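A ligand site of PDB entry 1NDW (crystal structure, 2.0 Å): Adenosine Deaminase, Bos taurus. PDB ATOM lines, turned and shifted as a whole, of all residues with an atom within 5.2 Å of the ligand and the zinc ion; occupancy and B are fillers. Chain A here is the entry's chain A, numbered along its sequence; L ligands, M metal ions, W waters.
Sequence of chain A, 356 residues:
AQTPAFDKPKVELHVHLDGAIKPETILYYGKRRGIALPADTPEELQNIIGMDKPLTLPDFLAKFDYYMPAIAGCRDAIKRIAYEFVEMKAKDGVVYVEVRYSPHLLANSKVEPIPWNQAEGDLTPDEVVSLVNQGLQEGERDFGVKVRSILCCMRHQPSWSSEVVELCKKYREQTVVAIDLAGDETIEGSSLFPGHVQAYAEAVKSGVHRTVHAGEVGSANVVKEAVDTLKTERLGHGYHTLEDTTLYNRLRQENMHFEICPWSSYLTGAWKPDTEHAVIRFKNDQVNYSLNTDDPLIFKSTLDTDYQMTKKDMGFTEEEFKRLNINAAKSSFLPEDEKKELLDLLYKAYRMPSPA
The side-chain carboxylate of Asp 295 sits at hydrogen-bond distance from a nitrogen (N2) of the ligand (2.8 Å).
O2 of the ligand is in hydrogen-bond range of OD2 of Asp 18 (2.8 Å).
ND1 of His 16 is in hydrogen-bond range of O2 of the ligand.
The indole nitrogen (NE1) of Trp 116 is in hydrogen-bond range of the backbone carbonyl oxygen (O) of Leu 105, at 2.6 Å.
A ring nitrogen (ND1) of His 14 sits close to the guanidinium group of Arg 100.
The side-chain hydroxyl (OG) of Ser 102 is in hydrogen-bond range of the backbone NH (N) of Leu 105, 3.3 Å away.
Merely in contact with the ligand: Leu 61, Phe 64, Leu 105, Met 154 and Trp 116.
Nine residues have an atom within 4 Å of the ligand: His 16, Asp 18, Leu 61, Phe 64, Leu 105, Trp 116, Met 154, Asp 294 and Asp 295.
The zinc ion is bound by NE2 of His 16, water W2, NE2 of His 14, NE2 of His 213 and OD2 of Asp 294.
Water W2 lies within hydrogen-bond range of the side-chain carboxylate of Asp 294 (2.5 Å) and a ring nitrogen (NE2) of His 237 (2.7 Å).
Water W4 bridges O1 of the ligand (2.8 Å) and N of Gly 183 (2.8 Å).
Water W1 bridges a nitrogen (N3) of the ligand and the side-chain carboxylate of Asp 294.
Water W8 bridges O1 of the ligand (3.5 Å) and O of Gly 183 (3.5 Å).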
ATOM      1  N   HIS A  14      34.700  18.080 -18.235  1.00  0.00           N
ATOM      2  CA  HIS A  14      33.737  18.500 -17.187  1.00  0.00           C
ATOM      3  C   HIS A  14      32.908  17.325 -16.524  1.00  0.00           C
ATOM      4  O   HIS A  14      31.794  17.082 -16.897  1.00  0.00           O
ATOM      5  CB  HIS A  14      32.785  19.638 -17.721  1.00  0.00           C
ATOM      6  CG  HIS A  14      32.056  20.439 -16.624  1.00  0.00           C
ATOM      7  ND1 HIS A  14      32.158  21.730 -16.432  1.00  0.00           N
ATOM      8  CD2 HIS A  14      31.210  20.038 -15.582  1.00  0.00           C
ATOM      9  CE1 HIS A  14      31.404  22.079 -15.323  1.00  0.00           C
ATOM     10  NE2 HIS A  14      30.789  21.072 -14.761  1.00  0.00           N
ATOM     11  N   HIS A  16      32.366  15.736 -12.279  1.00  0.00           N
ATOM     12  CA  HIS A  16      32.751  15.919 -10.898  1.00  0.00           C
ATOM     13  C   HIS A  16      32.946  14.540 -10.251  1.00  0.00           C
ATOM     14  O   HIS A  16      32.010  13.751 -10.262  1.00  0.00           O
ATOM     15  CB  HIS A  16      31.508  16.615 -10.038  1.00  0.00           C
ATOM     16  CG  HIS A  16      31.103  18.007 -10.559  1.00  0.00           C
ATOM     17  ND1 HIS A  16      31.414  19.070  -9.805  1.00  0.00           N
ATOM     18  CD2 HIS A  16      30.578  18.500 -11.729  1.00  0.00           C
ATOM     19  CE1 HIS A  16      31.070  20.209 -10.496  1.00  0.00           C
ATOM     20  NE2 HIS A  16      30.563  19.936 -11.698  1.00  0.00           N
ATOM     21  N   ASP A  18      32.744  13.604  -7.222  1.00  0.00           N
ATOM     22  CA  ASP A  18      31.657  13.380  -6.223  1.00  0.00           C
ATOM     23  C   ASP A  18      30.307  13.168  -6.751  1.00  0.00           C
ATOM     24  O   ASP A  18      29.412  12.778  -6.011  1.00  0.00           O
ATOM     25  CB  ASP A  18      31.574  14.414  -5.059  1.00  0.00           C
ATOM     26  CG  ASP A  18      31.736  15.847  -5.563  1.00  0.00           C
ATOM     27  OD1 ASP A  18      31.769  16.733  -4.752  1.00  0.00           O
ATOM     28  OD2 ASP A  18      31.869  16.133  -6.761  1.00  0.00           O
ATOM     29  N   GLY A  19      30.193  13.429  -8.006  1.00  0.00           N
ATOM     30  CA  GLY A  19      28.982  13.019  -8.677  1.00  0.00           C
ATOM     31  C   GLY A  19      29.154  11.874  -9.658  1.00  0.00           C
ATOM     32  O   GLY A  19      28.351  11.722 -10.573  1.00  0.00           O
ATOM     33  N   PHE A  60      17.754  18.762  -5.372  1.00  0.00           N
ATOM     34  CA  PHE A  60      19.085  18.316  -5.943  1.00  0.00           C
ATOM     35  C   PHE A  60      20.234  18.208  -4.978  1.00  0.00           C
ATOM     36  O   PHE A  60      20.872  17.189  -4.827  1.00  0.00           O
ATOM     37  CB  PHE A  60      19.505  19.307  -7.062  1.00  0.00           C
ATOM     38  CG  PHE A  60      20.803  18.887  -7.695  1.00  0.00           C
ATOM     39  CD1 PHE A  60      20.837  17.722  -8.503  1.00  0.00           C
ATOM     40  CD2 PHE A  60      21.943  19.686  -7.492  1.00  0.00           C
ATOM     41  CE1 PHE A  60      21.982  17.471  -9.271  1.00  0.00           C
ATOM     42  CE2 PHE A  60      23.084  19.389  -8.298  1.00  0.00           C
ATOM     43  CZ  PHE A  60      23.027  18.366  -9.226  1.00  0.00           C
ATOM     44  N   LEU A  61      20.483  19.305  -4.217  1.00  0.00           N
ATOM     45  CA  LEU A  61      21.508  19.227  -3.192  1.00  0.00           C
ATOM     46  C   LEU A  61      21.391  18.126  -2.101  1.00  0.00           C
ATOM     47  O   LEU A  61      22.357  17.471  -1.664  1.00  0.00           O
ATOM     48  CB  LEU A  61      21.589  20.640  -2.544  1.00  0.00           C
ATOM     49  CG  LEU A  61      22.112  21.792  -3.452  1.00  0.00           C
ATOM     50  CD1 LEU A  61      21.876  22.996  -2.628  1.00  0.00           C
ATOM     51  CD2 LEU A  61      23.606  21.935  -3.719  1.00  0.00           C
ATOM     52  N   PHE A  64      23.295  14.861  -2.222  1.00  0.00           N
ATOM     53  CA  PHE A  64      24.676  14.652  -1.716  1.00  0.00           C
ATOM     54  C   PHE A  64      24.679  14.226  -0.176  1.00  0.00           C
ATOM     55  O   PHE A  64      25.555  13.555   0.378  1.00  0.00           O
ATOM     56  CB  PHE A  64      25.577  15.968  -2.054  1.00  0.00           C
ATOM     57  CG  PHE A  64      25.755  16.231  -3.547  1.00  0.00           C
ATOM     58  CD1 PHE A  64      24.813  17.006  -4.288  1.00  0.00           C
ATOM     59  CD2 PHE A  64      26.923  15.686  -4.177  1.00  0.00           C
ATOM     60  CE1 PHE A  64      25.120  17.323  -5.656  1.00  0.00           C
ATOM     61  CE2 PHE A  64      27.173  15.962  -5.572  1.00  0.00           C
ATOM     62  CZ  PHE A  64      26.278  16.781  -6.244  1.00  0.00           C
ATOM     63  N   ARG A 100      37.065  16.821 -11.523  1.00  0.00           N
ATOM     64  CA  ARG A 100      37.077  17.908 -10.571  1.00  0.00           C
ATOM     65  C   ARG A 100      36.267  17.553  -9.345  1.00  0.00           C
ATOM     66  O   ARG A 100      35.303  16.820  -9.404  1.00  0.00           O
ATOM     67  CB  ARG A 100      36.453  19.217 -11.160  1.00  0.00           C
ATOM     68  CG  ARG A 100      34.894  19.025 -11.538  1.00  0.00           C
ATOM     69  CD  ARG A 100      34.546  20.484 -12.138  1.00  0.00           C
ATOM     70  NE  ARG A 100      35.169  20.508 -13.512  1.00  0.00           N
ATOM     71  CZ  ARG A 100      35.105  21.576 -14.368  1.00  0.00           C
ATOM     72  NH1 ARG A 100      34.354  22.626 -13.988  1.00  0.00           N
ATOM     73  NH2 ARG A 100      35.677  21.558 -15.628  1.00  0.00           N
ATOM     74  N   TYR A 101      36.687  18.167  -8.235  1.00  0.00           N
ATOM     75  CA  TYR A 101      36.006  17.973  -6.983  1.00  0.00           C
ATOM     76  C   TYR A 101      36.537  19.007  -5.967  1.00  0.00           C
ATOM     77  O   TYR A 101      37.590  19.617  -6.109  1.00  0.00           O
ATOM     78  CB  TYR A 101      36.277  16.529  -6.331  1.00  0.00           C
ATOM     79  CG  TYR A 101      37.756  16.390  -6.027  1.00  0.00           C
ATOM     80  CD1 TYR A 101      38.185  16.439  -4.674  1.00  0.00           C
ATOM     81  CD2 TYR A 101      38.721  16.136  -7.097  1.00  0.00           C
ATOM     82  CE1 TYR A 101      39.513  16.270  -4.334  1.00  0.00           C
ATOM     83  CE2 TYR A 101      40.083  15.990  -6.753  1.00  0.00           C
ATOM     84  CZ  TYR A 101      40.445  16.042  -5.392  1.00  0.00           C
ATOM     85  OH  TYR A 101      41.803  15.967  -5.051  1.00  0.00           O
ATOM     86  N   SER A 102      35.692  19.218  -4.872  1.00  0.00           N
ATOM     87  CA  SER A 102      36.167  20.052  -3.777  1.00  0.00           C
ATOM     88  C   SER A 102      36.722  19.096  -2.681  1.00  0.00           C
ATOM     89  O   SER A 102      36.052  18.260  -2.079  1.00  0.00           O
ATOM     90  CB  SER A 102      34.873  20.854  -3.174  1.00  0.00           C
ATOM     91  OG  SER A 102      35.312  21.236  -1.798  1.00  0.00           O
ATOM     92  N   LEU A 105      35.181  19.152   0.806  1.00  0.00           N
ATOM     93  CA  LEU A 105      33.925  18.460   0.964  1.00  0.00           C
ATOM     94  C   LEU A 105      34.005  16.897   1.203  1.00  0.00           C
ATOM     95  O   LEU A 105      33.037  16.243   1.560  1.00  0.00           O
ATOM     96  CB  LEU A 105      32.988  18.833  -0.211  1.00  0.00           C
ATOM     97  CG  LEU A 105      32.472  20.235  -0.336  1.00  0.00           C
ATOM     98  CD1 LEU A 105      31.518  20.286  -1.541  1.00  0.00           C
ATOM     99  CD2 LEU A 105      31.569  20.552   0.963  1.00  0.00           C
ATOM    100  N   TRP A 116      28.427  18.036   5.670  1.00  0.00           N
ATOM    101  CA  TRP A 116      27.511  16.892   5.734  1.00  0.00           C
ATOM    102  C   TRP A 116      27.217  16.474   7.169  1.00  0.00           C
ATOM    103  O   TRP A 116      27.073  15.299   7.457  1.00  0.00           O
ATOM    104  CB  TRP A 116      28.058  15.650   4.955  1.00  0.00           C
ATOM    105  CG  TRP A 116      28.780  16.096   3.675  1.00  0.00           C
ATOM    106  CD1 TRP A 116      30.142  15.948   3.432  1.00  0.00           C
ATOM    107  CD2 TRP A 116      28.267  16.657   2.467  1.00  0.00           C
ATOM    108  NE1 TRP A 116      30.489  16.315   2.162  1.00  0.00           N
ATOM    109  CE2 TRP A 116      29.365  16.759   1.545  1.00  0.00           C
ATOM    110  CE3 TRP A 116      27.010  17.182   2.101  1.00  0.00           C
ATOM    111  CZ2 TRP A 116      29.173  17.299   0.271  1.00  0.00           C
ATOM    112  CZ3 TRP A 116      26.850  17.813   0.849  1.00  0.00           C
ATOM    113  CH2 TRP A 116      27.937  17.837  -0.097  1.00  0.00           C
ATOM    114  N   CYS A 152      37.968  22.486  -6.840  1.00  0.00           N
ATOM    115  CA  CYS A 152      36.958  23.516  -6.892  1.00  0.00           C
ATOM    116  C   CYS A 152      36.982  24.316  -5.592  1.00  0.00           C
ATOM    117  O   CYS A 152      36.797  23.780  -4.514  1.00  0.00           O
ATOM    118  CB  CYS A 152      35.559  22.767  -6.921  1.00  0.00           C
ATOM    119  SG  CYS A 152      35.322  21.555  -8.323  1.00  0.00           S
ATOM    120  N   MET A 154      34.227  26.712  -3.690  1.00  0.00           N
ATOM    121  CA  MET A 154      32.693  26.711  -3.575  1.00  0.00           C
ATOM    122  C   MET A 154      32.165  28.147  -3.331  1.00  0.00           C
ATOM    123  O   MET A 154      32.684  28.821  -2.423  1.00  0.00           O
ATOM    124  CB  MET A 154      32.306  25.842  -2.443  1.00  0.00           C
ATOM    125  CG  MET A 154      32.629  24.221  -2.536  1.00  0.00           C
ATOM    126  SD  MET A 154      31.960  23.478  -4.022  1.00  0.00           S
ATOM    127  CE  MET A 154      30.216  23.781  -3.900  1.00  0.00           C
ATOM    128  N   HIS A 156      29.677  29.599  -2.011  1.00  0.00           N
ATOM    129  CA  HIS A 156      29.213  30.064  -0.673  1.00  0.00           C
ATOM    130  C   HIS A 156      30.234  30.083   0.375  1.00  0.00           C
ATOM    131  O   HIS A 156      29.975  30.420   1.543  1.00  0.00           O
ATOM    132  CB  HIS A 156      27.903  29.269  -0.274  1.00  0.00           C
ATOM    133  CG  HIS A 156      28.376  27.884  -0.023  1.00  0.00           C
ATOM    134  ND1 HIS A 156      28.593  27.010  -1.021  1.00  0.00           N
ATOM    135  CD2 HIS A 156      28.668  27.299   1.206  1.00  0.00           C
ATOM    136  CE1 HIS A 156      29.024  25.846  -0.448  1.00  0.00           C
ATOM    137  NE2 HIS A 156      29.061  26.042   0.898  1.00  0.00           N
ATOM    138  N   ALA A 182      32.746  26.305  -8.171  1.00  0.00           N
ATOM    139  CA  ALA A 182      31.554  25.452  -8.320  1.00  0.00           C
ATOM    140  C   ALA A 182      30.559  25.898  -7.201  1.00  0.00           C
ATOM    141  O   ALA A 182      30.858  26.718  -6.389  1.00  0.00           O
ATOM    142  CB  ALA A 182      31.936  23.859  -8.029  1.00  0.00           C
ATOM    143  N   GLY A 183      29.309  25.395  -7.281  1.00  0.00           N
ATOM    144  CA  GLY A 183      28.099  25.604  -6.403  1.00  0.00           C
ATOM    145  C   GLY A 183      27.063  26.561  -6.934  1.00  0.00           C
ATOM    146  O   GLY A 183      26.671  26.565  -8.079  1.00  0.00           O
ATOM    147  N   HIS A 213      32.451  27.630 -13.151  1.00  0.00           N
ATOM    148  CA  HIS A 213      31.070  27.457 -13.678  1.00  0.00           C
ATOM    149  C   HIS A 213      30.229  28.764 -13.852  1.00  0.00           C
ATOM    150  O   HIS A 213      30.032  29.518 -12.914  1.00  0.00           O
ATOM    151  CB  HIS A 213      30.274  26.540 -12.619  1.00  0.00           C
ATOM    152  CG  HIS A 213      30.749  25.088 -12.592  1.00  0.00           C
ATOM    153  ND1 HIS A 213      31.940  24.657 -12.150  1.00  0.00           N
ATOM    154  CD2 HIS A 213      29.880  23.966 -12.712  1.00  0.00           C
ATOM    155  CE1 HIS A 213      31.796  23.386 -11.966  1.00  0.00           C
ATOM    156  NE2 HIS A 213      30.546  22.903 -12.248  1.00  0.00           N
ATOM    157  N   HIS A 237      29.574  25.109 -18.767  1.00  0.00           N
ATOM    158  CA  HIS A 237      28.303  25.445 -19.440  1.00  0.00           C
ATOM    159  C   HIS A 237      28.302  26.725 -20.247  1.00  0.00           C
ATOM    160  O   HIS A 237      28.500  26.816 -21.457  1.00  0.00           O
ATOM    161  CB  HIS A 237      27.121  25.460 -18.405  1.00  0.00           C
ATOM    162  CG  HIS A 237      27.069  24.243 -17.511  1.00  0.00           C
ATOM    163  ND1 HIS A 237      26.469  23.048 -17.778  1.00  0.00           N
ATOM    164  CD2 HIS A 237      27.557  24.080 -16.263  1.00  0.00           C
ATOM    165  CE1 HIS A 237      26.603  22.192 -16.804  1.00  0.00           C
ATOM    166  NE2 HIS A 237      27.261  22.785 -15.815  1.00  0.00           N
ATOM    167  N   ASP A 294      29.065  15.836 -16.487  1.00  0.00           N
ATOM    168  CA  ASP A 294      28.848  16.532 -15.182  1.00  0.00           C
ATOM    169  C   ASP A 294      28.840  15.602 -13.944  1.00  0.00           C
ATOM    170  O   ASP A 294      29.783  15.481 -13.157  1.00  0.00           O
ATOM    171  CB  ASP A 294      27.582  17.442 -15.485  1.00  0.00           C
ATOM    172  CG  ASP A 294      27.593  18.666 -14.569  1.00  0.00           C
ATOM    173  OD1 ASP A 294      26.596  19.456 -14.578  1.00  0.00           O
ATOM    174  OD2 ASP A 294      28.612  18.804 -13.904  1.00  0.00           O
ATOM    175  N   ASP A 295      27.657  14.826 -13.793  1.00  0.00           N
ATOM    176  CA  ASP A 295      27.406  14.012 -12.601  1.00  0.00           C
ATOM    177  C   ASP A 295      26.659  12.683 -13.082  1.00  0.00           C
ATOM    178  O   ASP A 295      25.426  12.519 -12.976  1.00  0.00           O
ATOM    179  CB  ASP A 295      26.502  14.720 -11.542  1.00  0.00           C
ATOM    180  CG  ASP A 295      27.152  15.968 -11.124  1.00  0.00           C
ATOM    181  OD1 ASP A 295      27.736  15.922 -10.048  1.00  0.00           O
ATOM    182  OD2 ASP A 295      27.162  16.913 -11.919  1.00  0.00           O
HETATM  183  C1  LIG L   1      28.718  20.220  -7.694  1.00  0.00           C
HETATM  184  N1  LIG L   1      29.502  19.149  -7.104  1.00  0.00           N
HETATM  185  C2  LIG L   1      29.290  18.057  -7.805  1.00  0.00           C
HETATM  186  N2  LIG L   1      28.461  18.256  -8.768  1.00  0.00           N
HETATM  187  C3  LIG L   1      28.079  19.642  -8.706  1.00  0.00           C
HETATM  188  C4  LIG L   1      27.197  20.349  -9.636  1.00  0.00           C
HETATM  189  O1  LIG L   1      26.911  21.551  -9.498  1.00  0.00           O
HETATM  190  N3  LIG L   1      26.607  19.658 -10.606  1.00  0.00           N
HETATM  191  C5  LIG L   1      30.253  19.232  -5.838  1.00  0.00           C
HETATM  192  C6  LIG L   1      31.682  19.782  -6.086  1.00  0.00           C
HETATM  193  O2  LIG L   1      32.070  18.910  -7.195  1.00  0.00           O
HETATM  194  C7  LIG L   1      29.583  20.023  -4.708  1.00  0.00           C
HETATM  195  C8  LIG L   1      28.126  19.530  -4.449  1.00  0.00           C
HETATM  196  C9  LIG L   1      27.481  20.146  -3.220  1.00  0.00           C
HETATM  197  C10 LIG L   1      26.172  19.823  -2.922  1.00  0.00           C
HETATM  198  C11 LIG L   1      25.535  20.345  -1.802  1.00  0.00           C
HETATM  199  C12 LIG L   1      26.197  21.270  -0.990  1.00  0.00           C
HETATM  200  C13 LIG L   1      27.521  21.642  -1.269  1.00  0.00           C
HETATM  201  C14 LIG L   1      28.140  21.037  -2.385  1.00  0.00           C
HETATM  202 ZN    ZN M   1      29.729  20.984 -13.036  1.00  0.00          ZN
HETATM  203  O   HOH W   1      24.789  20.708 -12.511  1.00  0.00           O
HETATM  204  O   HOH W   2      27.922  21.380 -13.571  1.00  0.00           O
HETATM  205  O   HOH W   3      23.229  21.950  -0.168  1.00  0.00           O
HETATM  206  O   HOH W   4      28.911  23.453  -9.326  1.00  0.00           O
HETATM  207  O   HOH W   5      28.189  20.394   1.488  1.00  0.00           O
HETATM  208  O   HOH W   6      26.758  22.452  -4.949  1.00  0.00           O
HETATM  209  O   HOH W   7      26.618  23.416 -11.666  1.00  0.00           O
HETATM  210  O   HOH W   8      24.571  23.794  -8.275  1.00  0.00           O
